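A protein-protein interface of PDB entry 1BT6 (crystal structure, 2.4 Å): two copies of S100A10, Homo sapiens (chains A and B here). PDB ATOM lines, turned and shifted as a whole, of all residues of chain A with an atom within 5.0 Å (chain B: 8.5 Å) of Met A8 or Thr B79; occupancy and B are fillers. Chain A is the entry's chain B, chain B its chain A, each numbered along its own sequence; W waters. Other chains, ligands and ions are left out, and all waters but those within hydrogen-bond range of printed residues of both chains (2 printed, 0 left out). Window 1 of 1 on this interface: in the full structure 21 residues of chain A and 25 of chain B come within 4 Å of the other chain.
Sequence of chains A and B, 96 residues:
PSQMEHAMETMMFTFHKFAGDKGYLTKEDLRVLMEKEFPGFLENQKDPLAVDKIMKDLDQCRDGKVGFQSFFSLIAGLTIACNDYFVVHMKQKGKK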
ATOM      1  N   GLN A   3      11.569 -12.572 -27.375  1.00  0.00           N
ATOM      2  CA  GLN A   3      10.609 -11.633 -26.736  1.00  0.00           C
ATOM      3  C   GLN A   3      11.309 -10.392 -26.234  1.00  0.00           C
ATOM      4  O   GLN A   3      10.834  -9.275 -26.296  1.00  0.00           O
ATOM      5  CB  GLN A   3       9.988 -12.398 -25.571  1.00  0.00           C
ATOM      6  CG  GLN A   3       8.704 -13.138 -25.989  1.00  0.00           C
ATOM      7  CD  GLN A   3       8.100 -13.717 -24.688  1.00  0.00           C
ATOM      8  OE1 GLN A   3       8.688 -14.613 -24.079  1.00  0.00           O
ATOM      9  NE2 GLN A   3       7.000 -13.145 -24.240  1.00  0.00           N
ATOM     10  N   MET A   4      12.473 -10.505 -25.626  1.00  0.00           N
ATOM     11  CA  MET A   4      13.264  -9.386 -25.062  1.00  0.00           C
ATOM     12  C   MET A   4      13.568  -8.380 -26.151  1.00  0.00           C
ATOM     13  O   MET A   4      13.349  -7.207 -25.981  1.00  0.00           O
ATOM     14  CB  MET A   4      14.486  -9.911 -24.390  1.00  0.00           C
ATOM     15  CG  MET A   4      14.403 -10.175 -22.895  1.00  0.00           C
ATOM     16  SD  MET A   4      13.500  -9.119 -21.879  1.00  0.00           S
ATOM     17  CE  MET A   4      14.389  -7.848 -21.126  1.00  0.00           C
ATOM     18  N   GLU A   5      13.948  -8.833 -27.330  1.00  0.00           N
ATOM     19  CA  GLU A   5      14.216  -7.966 -28.440  1.00  0.00           C
ATOM     20  C   GLU A   5      12.973  -7.256 -28.944  1.00  0.00           C
ATOM     21  O   GLU A   5      13.101  -6.048 -29.153  1.00  0.00           O
ATOM     22  CB  GLU A   5      14.828  -8.731 -29.643  1.00  0.00           C
ATOM     23  CG  GLU A   5      16.222  -9.250 -29.284  1.00  0.00           C
ATOM     24  CD  GLU A   5      16.776 -10.115 -30.415  1.00  0.00           C
ATOM     25  OE1 GLU A   5      16.052 -10.867 -31.091  1.00  0.00           O
ATOM     26  OE2 GLU A   5      17.992 -10.070 -30.658  1.00  0.00           O
ATOM     27  N   HIS A   6      11.795  -7.970 -28.961  1.00  0.00           N
ATOM     28  CA  HIS A   6      10.550  -7.282 -29.345  1.00  0.00           C
ATOM     29  C   HIS A   6      10.218  -6.280 -28.294  1.00  0.00           C
ATOM     30  O   HIS A   6       9.813  -5.189 -28.645  1.00  0.00           O
ATOM     31  CB  HIS A   6       9.351  -8.220 -29.457  1.00  0.00           C
ATOM     32  CG  HIS A   6       9.328  -8.886 -30.802  1.00  0.00           C
ATOM     33  ND1 HIS A   6       8.776  -8.210 -31.872  1.00  0.00           N
ATOM     34  CD2 HIS A   6       9.814 -10.055 -31.181  1.00  0.00           C
ATOM     35  CE1 HIS A   6       8.933  -9.009 -32.960  1.00  0.00           C
ATOM     36  NE2 HIS A   6       9.545 -10.120 -32.563  1.00  0.00           N
ATOM     37  N   ALA A   7      10.425  -6.645 -27.040  1.00  0.00           N
ATOM     38  CA  ALA A   7      10.113  -5.627 -26.044  1.00  0.00           C
ATOM     39  C   ALA A   7      10.963  -4.405 -26.144  1.00  0.00           C
ATOM     40  O   ALA A   7      10.499  -3.291 -25.759  1.00  0.00           O
ATOM     41  CB  ALA A   7      10.174  -6.222 -24.627  1.00  0.00           C
ATOM     42  N   MET A   8      12.232  -4.556 -26.456  1.00  0.00           N
ATOM     43  CA  MET A   8      13.219  -3.394 -26.439  1.00  0.00           C
ATOM     44  C   MET A   8      12.869  -2.534 -27.634  1.00  0.00           C
ATOM     45  O   MET A   8      12.849  -1.340 -27.584  1.00  0.00           O
ATOM     46  CB  MET A   8      14.653  -3.986 -26.631  1.00  0.00           C
ATOM     47  CG  MET A   8      15.220  -4.491 -25.326  1.00  0.00           C
ATOM     48  SD  MET A   8      16.696  -5.553 -25.501  1.00  0.00           S
ATOM     49  CE  MET A   8      17.806  -4.271 -26.240  1.00  0.00           C
ATOM     50  N   GLU A   9      12.586  -3.184 -28.759  1.00  0.00           N
ATOM     51  CA  GLU A   9      12.175  -2.457 -29.924  1.00  0.00           C
ATOM     52  C   GLU A   9      10.877  -1.675 -29.635  1.00  0.00           C
ATOM     53  O   GLU A   9      10.886  -0.489 -29.918  1.00  0.00           O
ATOM     54  CB  GLU A   9      11.865  -3.398 -31.106  1.00  0.00           C
ATOM     55  CG  GLU A   9      11.529  -2.624 -32.385  1.00  0.00           C
ATOM     56  CD  GLU A   9      11.724  -3.466 -33.619  1.00  0.00           C
ATOM     57  OE1 GLU A   9      12.775  -4.165 -33.743  1.00  0.00           O
ATOM     58  OE2 GLU A   9      10.860  -3.513 -34.555  1.00  0.00           O
ATOM     59  N   THR A  10       9.853  -2.282 -28.969  1.00  0.00           N
ATOM     60  CA  THR A  10       8.633  -1.578 -28.771  1.00  0.00           C
ATOM     61  C   THR A  10       8.904  -0.340 -27.954  1.00  0.00           C
ATOM     62  O   THR A  10       8.348   0.632 -28.405  1.00  0.00           O
ATOM     63  CB  THR A  10       7.275  -2.247 -28.430  1.00  0.00           C
ATOM     64  OG1 THR A  10       6.811  -2.004 -27.122  1.00  0.00           O
ATOM     65  CG2 THR A  10       7.212  -3.697 -28.727  1.00  0.00           C
ATOM     66  N   MET A  11       9.708  -0.349 -26.921  1.00  0.00           N
ATOM     67  CA  MET A  11      10.036   0.795 -26.122  1.00  0.00           C
ATOM     68  C   MET A  11      10.828   1.832 -26.905  1.00  0.00           C
ATOM     69  O   MET A  11      10.720   3.020 -26.555  1.00  0.00           O
ATOM     70  CB  MET A  11      10.745   0.493 -24.812  1.00  0.00           C
ATOM     71  CG  MET A  11      10.319  -0.780 -24.056  1.00  0.00           C
ATOM     72  SD  MET A  11      11.011  -0.727 -22.388  1.00  0.00           S
ATOM     73  CE  MET A  11      10.002  -1.825 -21.421  1.00  0.00           C
ATOM     74  N   MET A  12      11.645   1.458 -27.878  1.00  0.00           N
ATOM     75  CA  MET A  12      12.422   2.369 -28.677  1.00  0.00           C
ATOM     76  C   MET A  12      11.495   3.097 -29.664  1.00  0.00           C
ATOM     77  O   MET A  12      11.568   4.306 -29.868  1.00  0.00           O
ATOM     78  CB  MET A  12      13.415   1.577 -29.601  1.00  0.00           C
ATOM     79  CG  MET A  12      14.705   2.321 -29.905  1.00  0.00           C
ATOM     80  SD  MET A  12      15.976   1.270 -30.644  1.00  0.00           S
ATOM     81  CE  MET A  12      15.514   1.296 -32.341  1.00  0.00           C
ATOM     82  N   PHE A  68      15.658  10.245 -24.616  1.00  0.00           N
ATOM     83  CA  PHE A  68      15.596   8.828 -24.504  1.00  0.00           C
ATOM     84  C   PHE A  68      15.966   8.258 -23.153  1.00  0.00           C
ATOM     85  O   PHE A  68      15.233   7.328 -22.708  1.00  0.00           O
ATOM     86  CB  PHE A  68      16.411   8.080 -25.576  1.00  0.00           C
ATOM     87  CG  PHE A  68      16.044   6.652 -25.681  1.00  0.00           C
ATOM     88  CD1 PHE A  68      14.814   6.297 -26.308  1.00  0.00           C
ATOM     89  CD2 PHE A  68      16.874   5.641 -25.216  1.00  0.00           C
ATOM     90  CE1 PHE A  68      14.441   4.966 -26.401  1.00  0.00           C
ATOM     91  CE2 PHE A  68      16.513   4.297 -25.323  1.00  0.00           C
ATOM     92  CZ  PHE A  68      15.275   3.942 -25.890  1.00  0.00           C
ATOM     93  N   PHE A  72      13.657   6.248 -20.529  1.00  0.00           N
ATOM     94  CA  PHE A  72      14.021   4.966 -19.972  1.00  0.00           C
ATOM     95  C   PHE A  72      14.009   4.959 -18.458  1.00  0.00           C
ATOM     96  O   PHE A  72      13.698   3.992 -17.794  1.00  0.00           O
ATOM     97  CB  PHE A  72      15.520   4.531 -20.247  1.00  0.00           C
ATOM     98  CG  PHE A  72      15.362   3.044 -20.437  1.00  0.00           C
ATOM     99  CD1 PHE A  72      14.845   2.588 -21.612  1.00  0.00           C
ATOM    100  CD2 PHE A  72      15.695   2.175 -19.422  1.00  0.00           C
ATOM    101  CE1 PHE A  72      14.655   1.230 -21.811  1.00  0.00           C
ATOM    102  CE2 PHE A  72      15.521   0.819 -19.630  1.00  0.00           C
ATOM    103  CZ  PHE A  72      14.994   0.375 -20.833  1.00  0.00           C
ATOM    104  N   MET B   4       3.312  -0.689 -24.657  1.00  0.00           N
ATOM    105  CA  MET B   4       4.205  -0.397 -23.579  1.00  0.00           C
ATOM    106  C   MET B   4       3.949  -1.310 -22.406  1.00  0.00           C
ATOM    107  O   MET B   4       4.846  -1.961 -21.839  1.00  0.00           O
ATOM    108  CB  MET B   4       4.143   1.076 -23.148  1.00  0.00           C
ATOM    109  CG  MET B   4       5.018   2.023 -23.986  1.00  0.00           C
ATOM    110  SD  MET B   4       6.764   1.531 -24.151  1.00  0.00           S
ATOM    111  CE  MET B   4       7.248   1.217 -22.468  1.00  0.00           C
ATOM    112  N   ALA B   7       5.235  -4.605 -23.264  1.00  0.00           N
ATOM    113  CA  ALA B   7       6.704  -4.644 -23.205  1.00  0.00           C
ATOM    114  C   ALA B   7       7.161  -4.773 -21.799  1.00  0.00           C
ATOM    115  O   ALA B   7       8.094  -5.610 -21.557  1.00  0.00           O
ATOM    116  CB  ALA B   7       7.274  -3.481 -24.031  1.00  0.00           C
ATOM    117  N   MET B   8       6.578  -4.036 -20.849  1.00  0.00           N
ATOM    118  CA  MET B   8       7.036  -4.125 -19.451  1.00  0.00           C
ATOM    119  C   MET B   8       6.777  -5.452 -18.782  1.00  0.00           C
ATOM    120  O   MET B   8       7.494  -5.995 -17.934  1.00  0.00           O
ATOM    121  CB  MET B   8       6.329  -3.035 -18.646  1.00  0.00           C
ATOM    122  CG  MET B   8       6.447  -1.640 -19.236  1.00  0.00           C
ATOM    123  SD  MET B   8       5.676  -0.264 -18.374  1.00  0.00           S
ATOM    124  CE  MET B   8       5.427  -0.729 -16.713  1.00  0.00           C
ATOM    125  N   THR B  10       6.482  -8.307 -20.433  1.00  0.00           N
ATOM    126  CA  THR B  10       7.413  -9.245 -20.990  1.00  0.00           C
ATOM    127  C   THR B  10       8.814  -9.173 -20.361  1.00  0.00           C
ATOM    128  O   THR B  10       9.311 -10.217 -19.895  1.00  0.00           O
ATOM    129  CB  THR B  10       7.401  -9.567 -22.441  1.00  0.00           C
ATOM    130  OG1 THR B  10       8.695  -9.550 -22.965  1.00  0.00           O
ATOM    131  CG2 THR B  10       6.322  -8.974 -23.282  1.00  0.00           C
ATOM    132  N   MET B  11       9.329  -8.008 -19.989  1.00  0.00           N
ATOM    133  CA  MET B  11      10.609  -7.951 -19.317  1.00  0.00           C
ATOM    134  C   MET B  11      10.537  -8.488 -17.921  1.00  0.00           C
ATOM    135  O   MET B  11      11.542  -9.021 -17.442  1.00  0.00           O
ATOM    136  CB  MET B  11      11.187  -6.518 -19.272  1.00  0.00           C
ATOM    137  CG  MET B  11      11.488  -6.004 -20.730  1.00  0.00           C
ATOM    138  SD  MET B  11      12.365  -4.433 -20.508  1.00  0.00           S
ATOM    139  CE  MET B  11      12.678  -3.986 -22.202  1.00  0.00           C
ATOM    140  N   GLU B  37      17.828 -15.067 -25.068  1.00  0.00           N
ATOM    141  CA  GLU B  37      17.287 -13.746 -25.505  1.00  0.00           C
ATOM    142  C   GLU B  37      18.427 -13.091 -26.177  1.00  0.00           C
ATOM    143  O   GLU B  37      19.580 -13.370 -25.649  1.00  0.00           O
ATOM    144  CB  GLU B  37      16.802 -13.002 -24.232  1.00  0.00           C
ATOM    145  CG  GLU B  37      15.673 -13.699 -23.503  1.00  0.00           C
ATOM    146  CD  GLU B  37      14.352 -13.701 -24.276  1.00  0.00           C
ATOM    147  OE1 GLU B  37      13.972 -12.909 -25.193  1.00  0.00           O
ATOM    148  OE2 GLU B  37      13.551 -14.595 -23.944  1.00  0.00           O
ATOM    149  N   PHE B  38      18.552 -12.333 -27.211  1.00  0.00           N
ATOM    150  CA  PHE B  38      19.925 -11.850 -27.613  1.00  0.00           C
ATOM    151  C   PHE B  38      20.938 -12.902 -27.999  1.00  0.00           C
ATOM    152  O   PHE B  38      22.178 -12.827 -27.725  1.00  0.00           O
ATOM    153  CB  PHE B  38      20.583 -10.908 -26.607  1.00  0.00           C
ATOM    154  CG  PHE B  38      19.770 -10.116 -25.658  1.00  0.00           C
ATOM    155  CD1 PHE B  38      18.826  -9.171 -26.101  1.00  0.00           C
ATOM    156  CD2 PHE B  38      19.834 -10.357 -24.293  1.00  0.00           C
ATOM    157  CE1 PHE B  38      18.059  -8.489 -25.183  1.00  0.00           C
ATOM    158  CE2 PHE B  38      19.065  -9.680 -23.383  1.00  0.00           C
ATOM    159  CZ  PHE B  38      18.167  -8.735 -23.825  1.00  0.00           C
ATOM    160  N   PHE B  41      23.906 -11.368 -30.233  1.00  0.00           N
ATOM    161  CA  PHE B  41      24.781 -10.409 -29.590  1.00  0.00           C
ATOM    162  C   PHE B  41      26.017 -11.034 -28.983  1.00  0.00           C
ATOM    163  O   PHE B  41      27.118 -10.497 -29.234  1.00  0.00           O
ATOM    164  CB  PHE B  41      23.977  -9.624 -28.583  1.00  0.00           C
ATOM    165  CG  PHE B  41      24.704  -8.630 -27.763  1.00  0.00           C
ATOM    166  CD1 PHE B  41      25.150  -7.449 -28.307  1.00  0.00           C
ATOM    167  CD2 PHE B  41      24.934  -8.917 -26.425  1.00  0.00           C
ATOM    168  CE1 PHE B  41      25.824  -6.541 -27.491  1.00  0.00           C
ATOM    169  CE2 PHE B  41      25.617  -8.001 -25.621  1.00  0.00           C
ATOM    170  CZ  PHE B  41      26.044  -6.827 -26.158  1.00  0.00           C
ATOM    171  N   PHE B  71      19.285  -6.331 -13.251  1.00  0.00           N
ATOM    172  CA  PHE B  71      18.909  -6.825 -14.588  1.00  0.00           C
ATOM    173  C   PHE B  71      18.401  -5.653 -15.452  1.00  0.00           C
ATOM    174  O   PHE B  71      18.615  -5.536 -16.646  1.00  0.00           O
ATOM    175  CB  PHE B  71      17.830  -7.871 -14.375  1.00  0.00           C
ATOM    176  CG  PHE B  71      17.026  -8.240 -15.614  1.00  0.00           C
ATOM    177  CD1 PHE B  71      17.530  -9.089 -16.555  1.00  0.00           C
ATOM    178  CD2 PHE B  71      15.757  -7.734 -15.790  1.00  0.00           C
ATOM    179  CE1 PHE B  71      16.764  -9.399 -17.676  1.00  0.00           C
ATOM    180  CE2 PHE B  71      14.965  -8.038 -16.858  1.00  0.00           C
ATOM    181  CZ  PHE B  71      15.494  -8.875 -17.808  1.00  0.00           C
ATOM    182  N   PHE B  72      17.638  -4.707 -14.849  1.00  0.00           N
ATOM    183  CA  PHE B  72      17.095  -3.604 -15.543  1.00  0.00           C
ATOM    184  C   PHE B  72      18.112  -2.600 -16.023  1.00  0.00           C
ATOM    185  O   PHE B  72      17.920  -1.985 -17.104  1.00  0.00           O
ATOM    186  CB  PHE B  72      15.918  -2.971 -14.729  1.00  0.00           C
ATOM    187  CG  PHE B  72      14.862  -2.528 -15.722  1.00  0.00           C
ATOM    188  CD1 PHE B  72      13.867  -3.377 -16.117  1.00  0.00           C
ATOM    189  CD2 PHE B  72      14.900  -1.268 -16.252  1.00  0.00           C
ATOM    190  CE1 PHE B  72      12.901  -2.961 -17.009  1.00  0.00           C
ATOM    191  CE2 PHE B  72      13.980  -0.886 -17.206  1.00  0.00           C
ATOM    192  CZ  PHE B  72      12.974  -1.702 -17.581  1.00  0.00           C
ATOM    193  N   SER B  73      19.196  -2.476 -15.273  1.00  0.00           N
ATOM    194  CA  SER B  73      20.289  -1.575 -15.718  1.00  0.00           C
ATOM    195  C   SER B  73      20.983  -2.228 -16.921  1.00  0.00           C
ATOM    196  O   SER B  73      21.291  -1.612 -17.947  1.00  0.00           O
ATOM    197  CB  SER B  73      21.217  -1.250 -14.568  1.00  0.00           C
ATOM    198  OG  SER B  73      22.352  -2.066 -14.547  1.00  0.00           O
ATOM    199  N   LEU B  74      21.056  -3.551 -16.961  1.00  0.00           N
ATOM    200  CA  LEU B  74      21.570  -4.225 -18.085  1.00  0.00           C
ATOM    201  C   LEU B  74      20.683  -3.981 -19.252  1.00  0.00           C
ATOM    202  O   LEU B  74      21.264  -3.730 -20.336  1.00  0.00           O
ATOM    203  CB  LEU B  74      21.892  -5.734 -17.817  1.00  0.00           C
ATOM    204  CG  LEU B  74      22.130  -6.501 -19.128  1.00  0.00           C
ATOM    205  CD1 LEU B  74      23.438  -6.046 -19.779  1.00  0.00           C
ATOM    206  CD2 LEU B  74      22.093  -7.965 -18.923  1.00  0.00           C
ATOM    207  N   ILE B  75      19.350  -4.059 -19.191  1.00  0.00           N
ATOM    208  CA  ILE B  75      18.477  -3.839 -20.377  1.00  0.00           C
ATOM    209  C   ILE B  75      18.493  -2.391 -20.832  1.00  0.00           C
ATOM    210  O   ILE B  75      18.377  -2.103 -22.022  1.00  0.00           O
ATOM    211  CB  ILE B  75      17.000  -4.219 -20.007  1.00  0.00           C
ATOM    212  CG1 ILE B  75      16.817  -5.640 -19.515  1.00  0.00           C
ATOM    213  CG2 ILE B  75      16.064  -3.902 -21.163  1.00  0.00           C
ATOM    214  CD1 ILE B  75      17.547  -6.766 -20.200  1.00  0.00           C
ATOM    215  N   ALA B  76      18.578  -1.428 -19.929  1.00  0.00           N
ATOM    216  CA  ALA B  76      18.648  -0.014 -20.271  1.00  0.00           C
ATOM    217  C   ALA B  76      19.952   0.209 -21.093  1.00  0.00           C
ATOM    218  O   ALA B  76      19.941   0.534 -22.279  1.00  0.00           O
ATOM    219  CB  ALA B  76      18.742   0.860 -18.991  1.00  0.00           C
ATOM    220  N   GLY B  77      21.051  -0.130 -20.511  1.00  0.00           N
ATOM    221  CA  GLY B  77      22.393  -0.245 -21.190  1.00  0.00           C
ATOM    222  C   GLY B  77      22.246  -0.811 -22.550  1.00  0.00           C
ATOM    223  O   GLY B  77      22.652  -0.136 -23.491  1.00  0.00           O
ATOM    224  N   LEU B  78      21.662  -1.961 -22.857  1.00  0.00           N
ATOM    225  CA  LEU B  78      21.549  -2.297 -24.249  1.00  0.00           C
ATOM    226  C   LEU B  78      20.543  -1.431 -25.006  1.00  0.00           C
ATOM    227  O   LEU B  78      20.750  -1.259 -26.271  1.00  0.00           O
ATOM    228  CB  LEU B  78      21.093  -3.762 -24.369  1.00  0.00           C
ATOM    229  CG  LEU B  78      21.939  -4.802 -23.646  1.00  0.00           C
ATOM    230  CD1 LEU B  78      21.268  -6.154 -23.746  1.00  0.00           C
ATOM    231  CD2 LEU B  78      23.363  -4.876 -24.307  1.00  0.00           C
ATOM    232  N   THR B  79      19.458  -0.971 -24.378  1.00  0.00           N
ATOM    233  CA  THR B  79      18.420  -0.290 -25.169  1.00  0.00           C
ATOM    234  C   THR B  79      18.910   1.064 -25.626  1.00  0.00           C
ATOM    235  O   THR B  79      18.762   1.460 -26.772  1.00  0.00           O
ATOM    236  CB  THR B  79      17.003  -0.111 -24.482  1.00  0.00           C
ATOM    237  OG1 THR B  79      16.582  -1.472 -24.045  1.00  0.00           O
ATOM    238  CG2 THR B  79      16.024   0.098 -25.611  1.00  0.00           C
ATOM    239  N   ILE B  80      19.536   1.734 -24.692  1.00  0.00           N
ATOM    240  CA  ILE B  80      20.108   3.070 -24.980  1.00  0.00           C
ATOM    241  C   ILE B  80      21.208   2.901 -26.033  1.00  0.00           C
ATOM    242  O   ILE B  80      21.121   3.531 -27.121  1.00  0.00           O
ATOM    243  CB  ILE B  80      20.576   3.611 -23.631  1.00  0.00           C
ATOM    244  CG1 ILE B  80      19.413   3.899 -22.679  1.00  0.00           C
ATOM    245  CG2 ILE B  80      21.416   4.852 -23.851  1.00  0.00           C
ATOM    246  CD1 ILE B  80      19.811   4.365 -21.310  1.00  0.00           C
ATOM    247  N   ALA B  81      22.035   1.789 -26.013  1.00  0.00           N
ATOM    248  CA  ALA B  81      23.045   1.703 -27.061  1.00  0.00           C
ATOM    249  C   ALA B  81      22.353   1.483 -28.368  1.00  0.00           C
ATOM    250  O   ALA B  81      22.797   1.988 -29.394  1.00  0.00           O
ATOM    251  CB  ALA B  81      24.078   0.568 -26.893  1.00  0.00           C
ATOM    252  N   CYS B  82      21.294   0.657 -28.344  1.00  0.00           N
ATOM    253  CA  CYS B  82      20.596   0.385 -29.603  1.00  0.00           C
ATOM    254  C   CYS B  82      19.995   1.621 -30.210  1.00  0.00           C
ATOM    255  O   CYS B  82      19.984   1.741 -31.422  1.00  0.00           O
ATOM    256  CB  CYS B  82      19.435  -0.620 -29.331  1.00  0.00           C
ATOM    257  SG  CYS B  82      20.158  -2.288 -29.356  1.00  0.00           S
ATOM    258  N   ASN B  83      19.477   2.504 -29.406  1.00  0.00           N
ATOM    259  CA  ASN B  83      18.875   3.747 -29.855  1.00  0.00           C
ATOM    260  C   ASN B  83      19.927   4.746 -30.339  1.00  0.00           C
ATOM    261  O   ASN B  83      19.614   5.609 -31.195  1.00  0.00           O
ATOM    262  CB  ASN B  83      18.103   4.397 -28.641  1.00  0.00           C
ATOM    263  CG  ASN B  83      17.457   5.663 -29.152  1.00  0.00           C
ATOM    264  OD1 ASN B  83      17.701   6.708 -28.598  1.00  0.00           O
ATOM    265  ND2 ASN B  83      16.649   5.602 -30.192  1.00  0.00           N
ATOM    266  N   ASP B  84      21.077   4.837 -29.682  1.00  0.00           N
ATOM    267  CA  ASP B  84      22.152   5.796 -30.213  1.00  0.00           C
ATOM    268  C   ASP B  84      22.520   5.249 -31.599  1.00  0.00           C
ATOM    269  O   ASP B  84      22.450   5.976 -32.586  1.00  0.00           O
ATOM    270  CB  ASP B  84      23.323   5.832 -29.299  1.00  0.00           C
ATOM    271  CG  ASP B  84      23.194   6.625 -28.068  1.00  0.00           C
ATOM    272  OD1 ASP B  84      22.470   7.638 -27.887  1.00  0.00           O
ATOM    273  OD2 ASP B  84      23.887   6.303 -27.096  1.00  0.00           O
ATOM    274  N   TYR B  85      22.736   3.949 -31.764  1.00  0.00           N
ATOM    275  CA  TYR B  85      23.029   3.501 -33.117  1.00  0.00           C
ATOM    276  C   TYR B  85      21.939   3.797 -34.115  1.00  0.00           C
ATOM    277  O   TYR B  85      22.098   4.202 -35.264  1.00  0.00           O
ATOM    278  CB  TYR B  85      23.293   2.012 -33.091  1.00  0.00           C
ATOM    279  CG  TYR B  85      23.695   1.435 -34.410  1.00  0.00           C
ATOM    280  CD1 TYR B  85      22.818   1.208 -35.451  1.00  0.00           C
ATOM    281  CD2 TYR B  85      25.061   1.089 -34.565  1.00  0.00           C
ATOM    282  CE1 TYR B  85      23.225   0.653 -36.651  1.00  0.00           C
ATOM    283  CE2 TYR B  85      25.486   0.525 -35.761  1.00  0.00           C
ATOM    284  CZ  TYR B  85      24.578   0.338 -36.773  1.00  0.00           C
ATOM    285  OH  TYR B  85      25.056  -0.223 -37.933  1.00  0.00           O
ATOM    286  N   PHE B  86      20.687   3.514 -33.771  1.00  0.00           N
ATOM    287  CA  PHE B  86      19.546   3.717 -34.640  1.00  0.00           C
ATOM    288  C   PHE B  86      19.402   5.175 -34.980  1.00  0.00           C
ATOM    289  O   PHE B  86      19.155   5.432 -36.145  1.00  0.00           O
ATOM    290  CB  PHE B  86      18.241   3.168 -33.959  1.00  0.00           C
ATOM    291  CG  PHE B  86      16.940   3.700 -34.458  1.00  0.00           C
ATOM    292  CD1 PHE B  86      16.291   3.098 -35.505  1.00  0.00           C
ATOM    293  CD2 PHE B  86      16.367   4.819 -33.868  1.00  0.00           C
ATOM    294  CE1 PHE B  86      15.070   3.573 -35.997  1.00  0.00           C
ATOM    295  CE2 PHE B  86      15.153   5.309 -34.357  1.00  0.00           C
ATOM    296  CZ  PHE B  86      14.502   4.687 -35.424  1.00  0.00           C
HETATM  297  O   HOH W   1      20.763 -10.657 -30.244  1.00  0.00           O
HETATM  298  O   HOH W   2      11.978 -15.055 -26.547  1.00  0.00           O
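Hydrophobic or aromatic side chains of chain A that line the printed part of chain B: Met A4, Ala A7, Met A8, Met A11, Met A12, Phe A68 and Phe A72.
Along chain A the printed residues that touch a printed residue of chain B span positions 3 to 72.
Printed residues of chain B that touch a printed residue of chain A: Met B4, Ala B7, Thr B10, Met B11, Glu B37, Phe B38, Phe B71, Phe B72, Ile B75, Ala B76, Leu B78, Thr B79, Ile B80, Asn B83 and Phe B86.
Hydrophobic or aromatic side chains of chain B within 4 Å of the printed part of chain A: Met B4, Ala B7, Met B11, Phe B38, Phe B71, Phe B72, Ile B75, Ala B76, Leu B78, Ile B80 and Phe B86.
Among the printed residues, no Asp or Glu carboxylate lies within 4 Å of a Lys or Arg side-chain nitrogen of the other chain.
Printed residues of chain B within 4 Å of Met A8: Phe B38 (3.3 Å), Leu B78 (3.8 Å) and Thr B79 (3.6 Å).
Thr B79 touches just these residues of chain A: Met A8, Phe A68 and Phe A72.
Of the printed residues of chain A, Phe B72 touches Phe A72 (3.3 Å).
Of the printed residues of chain A, Ile B80 touches Phe A68 (3.8 Å).
Asp B84 touches none of the printed residues of chain A.
Cys B82 touches none of the printed residues of chain A.
The nearest residue of chain B that does not touch Met A8 is Met B11 (4.1 Å).
The nearest printed residue of chain A that does not touch Met B11 is Met A8 (4.1 Å).
Ala B7 touches its own counterpart, Ala A7.
Thr A10 touches Ala B7, but with the chains exchanged Ala A7 does not touch Thr B10 (4.003 Å).
Met B11 touches its own counterpart, Met A11.
Phe B72 touches its own counterpart, Phe A72.
6 positions are printed for both chains.
Of the 22 pairs that touch across the chains among the printed residues, 5 have their exchanged pair printed and touching as well.
Among the printed residues, merely in contact across the chains: Met A8 with Phe B38 (3.3 Å), Phe A72 with Ala B76 (3.3 Å), Phe A72 with Phe B72 (3.3 Å), Phe A68 with Asn B83 (3.4 Å), Thr A10 with Ala B7 (3.5 Å), Met A4 with Met B11 (3.5 Å), Met A4 with Ile B75 (3.5 Å), Met A12 with Phe B86 (3.5 Å), Met A11 with Met B11 (3.5 Å), Met A8 with Thr B79 (3.6 Å), Met A4 with Phe B71 (3.6 Å), Ala A7 with Ala B7 (3.7 Å), Phe A72 with Thr B79 (3.8 Å), Phe A68 with Ile B80 (3.8 Å), Met A8 with Leu B78 (3.8 Å), Met A12 with Asn B83 (3.8 Å), Met A11 with Met B4 (3.9 Å), Phe A68 with Thr B79 (3.9 Å), Met A4 with Phe B38 (3.9 Å) and Gln A3 with Thr B10 (3.97 Å).
The side-chain hydroxyl (OG1) of Thr B79 sits at hydrogen-bond distance from the backbone carbonyl oxygen (O) of Ile B75, at 2.8 Å.
The side-chain sulfur (SG) of Cys B82 is in hydrogen-bond range of the backbone carbonyl oxygen (O) of Leu B78, 3.3 Å away.
Water W2 bridges N of Gln A3 and OE2 of Glu B37.
Water W1 lies within hydrogen-bond range of the side-chain carboxylate of Glu A5 (2.9 Å) and the backbone NH of Phe B41 (3.2 Å).
The side-chain carboxylate (OE1) of Glu B37 is in hydrogen-bond range of the backbone NH (N) of Met A4.
N of Gln A3 lies within hydrogen-bond range of OE1 of Glu B37 (3.3 Å).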
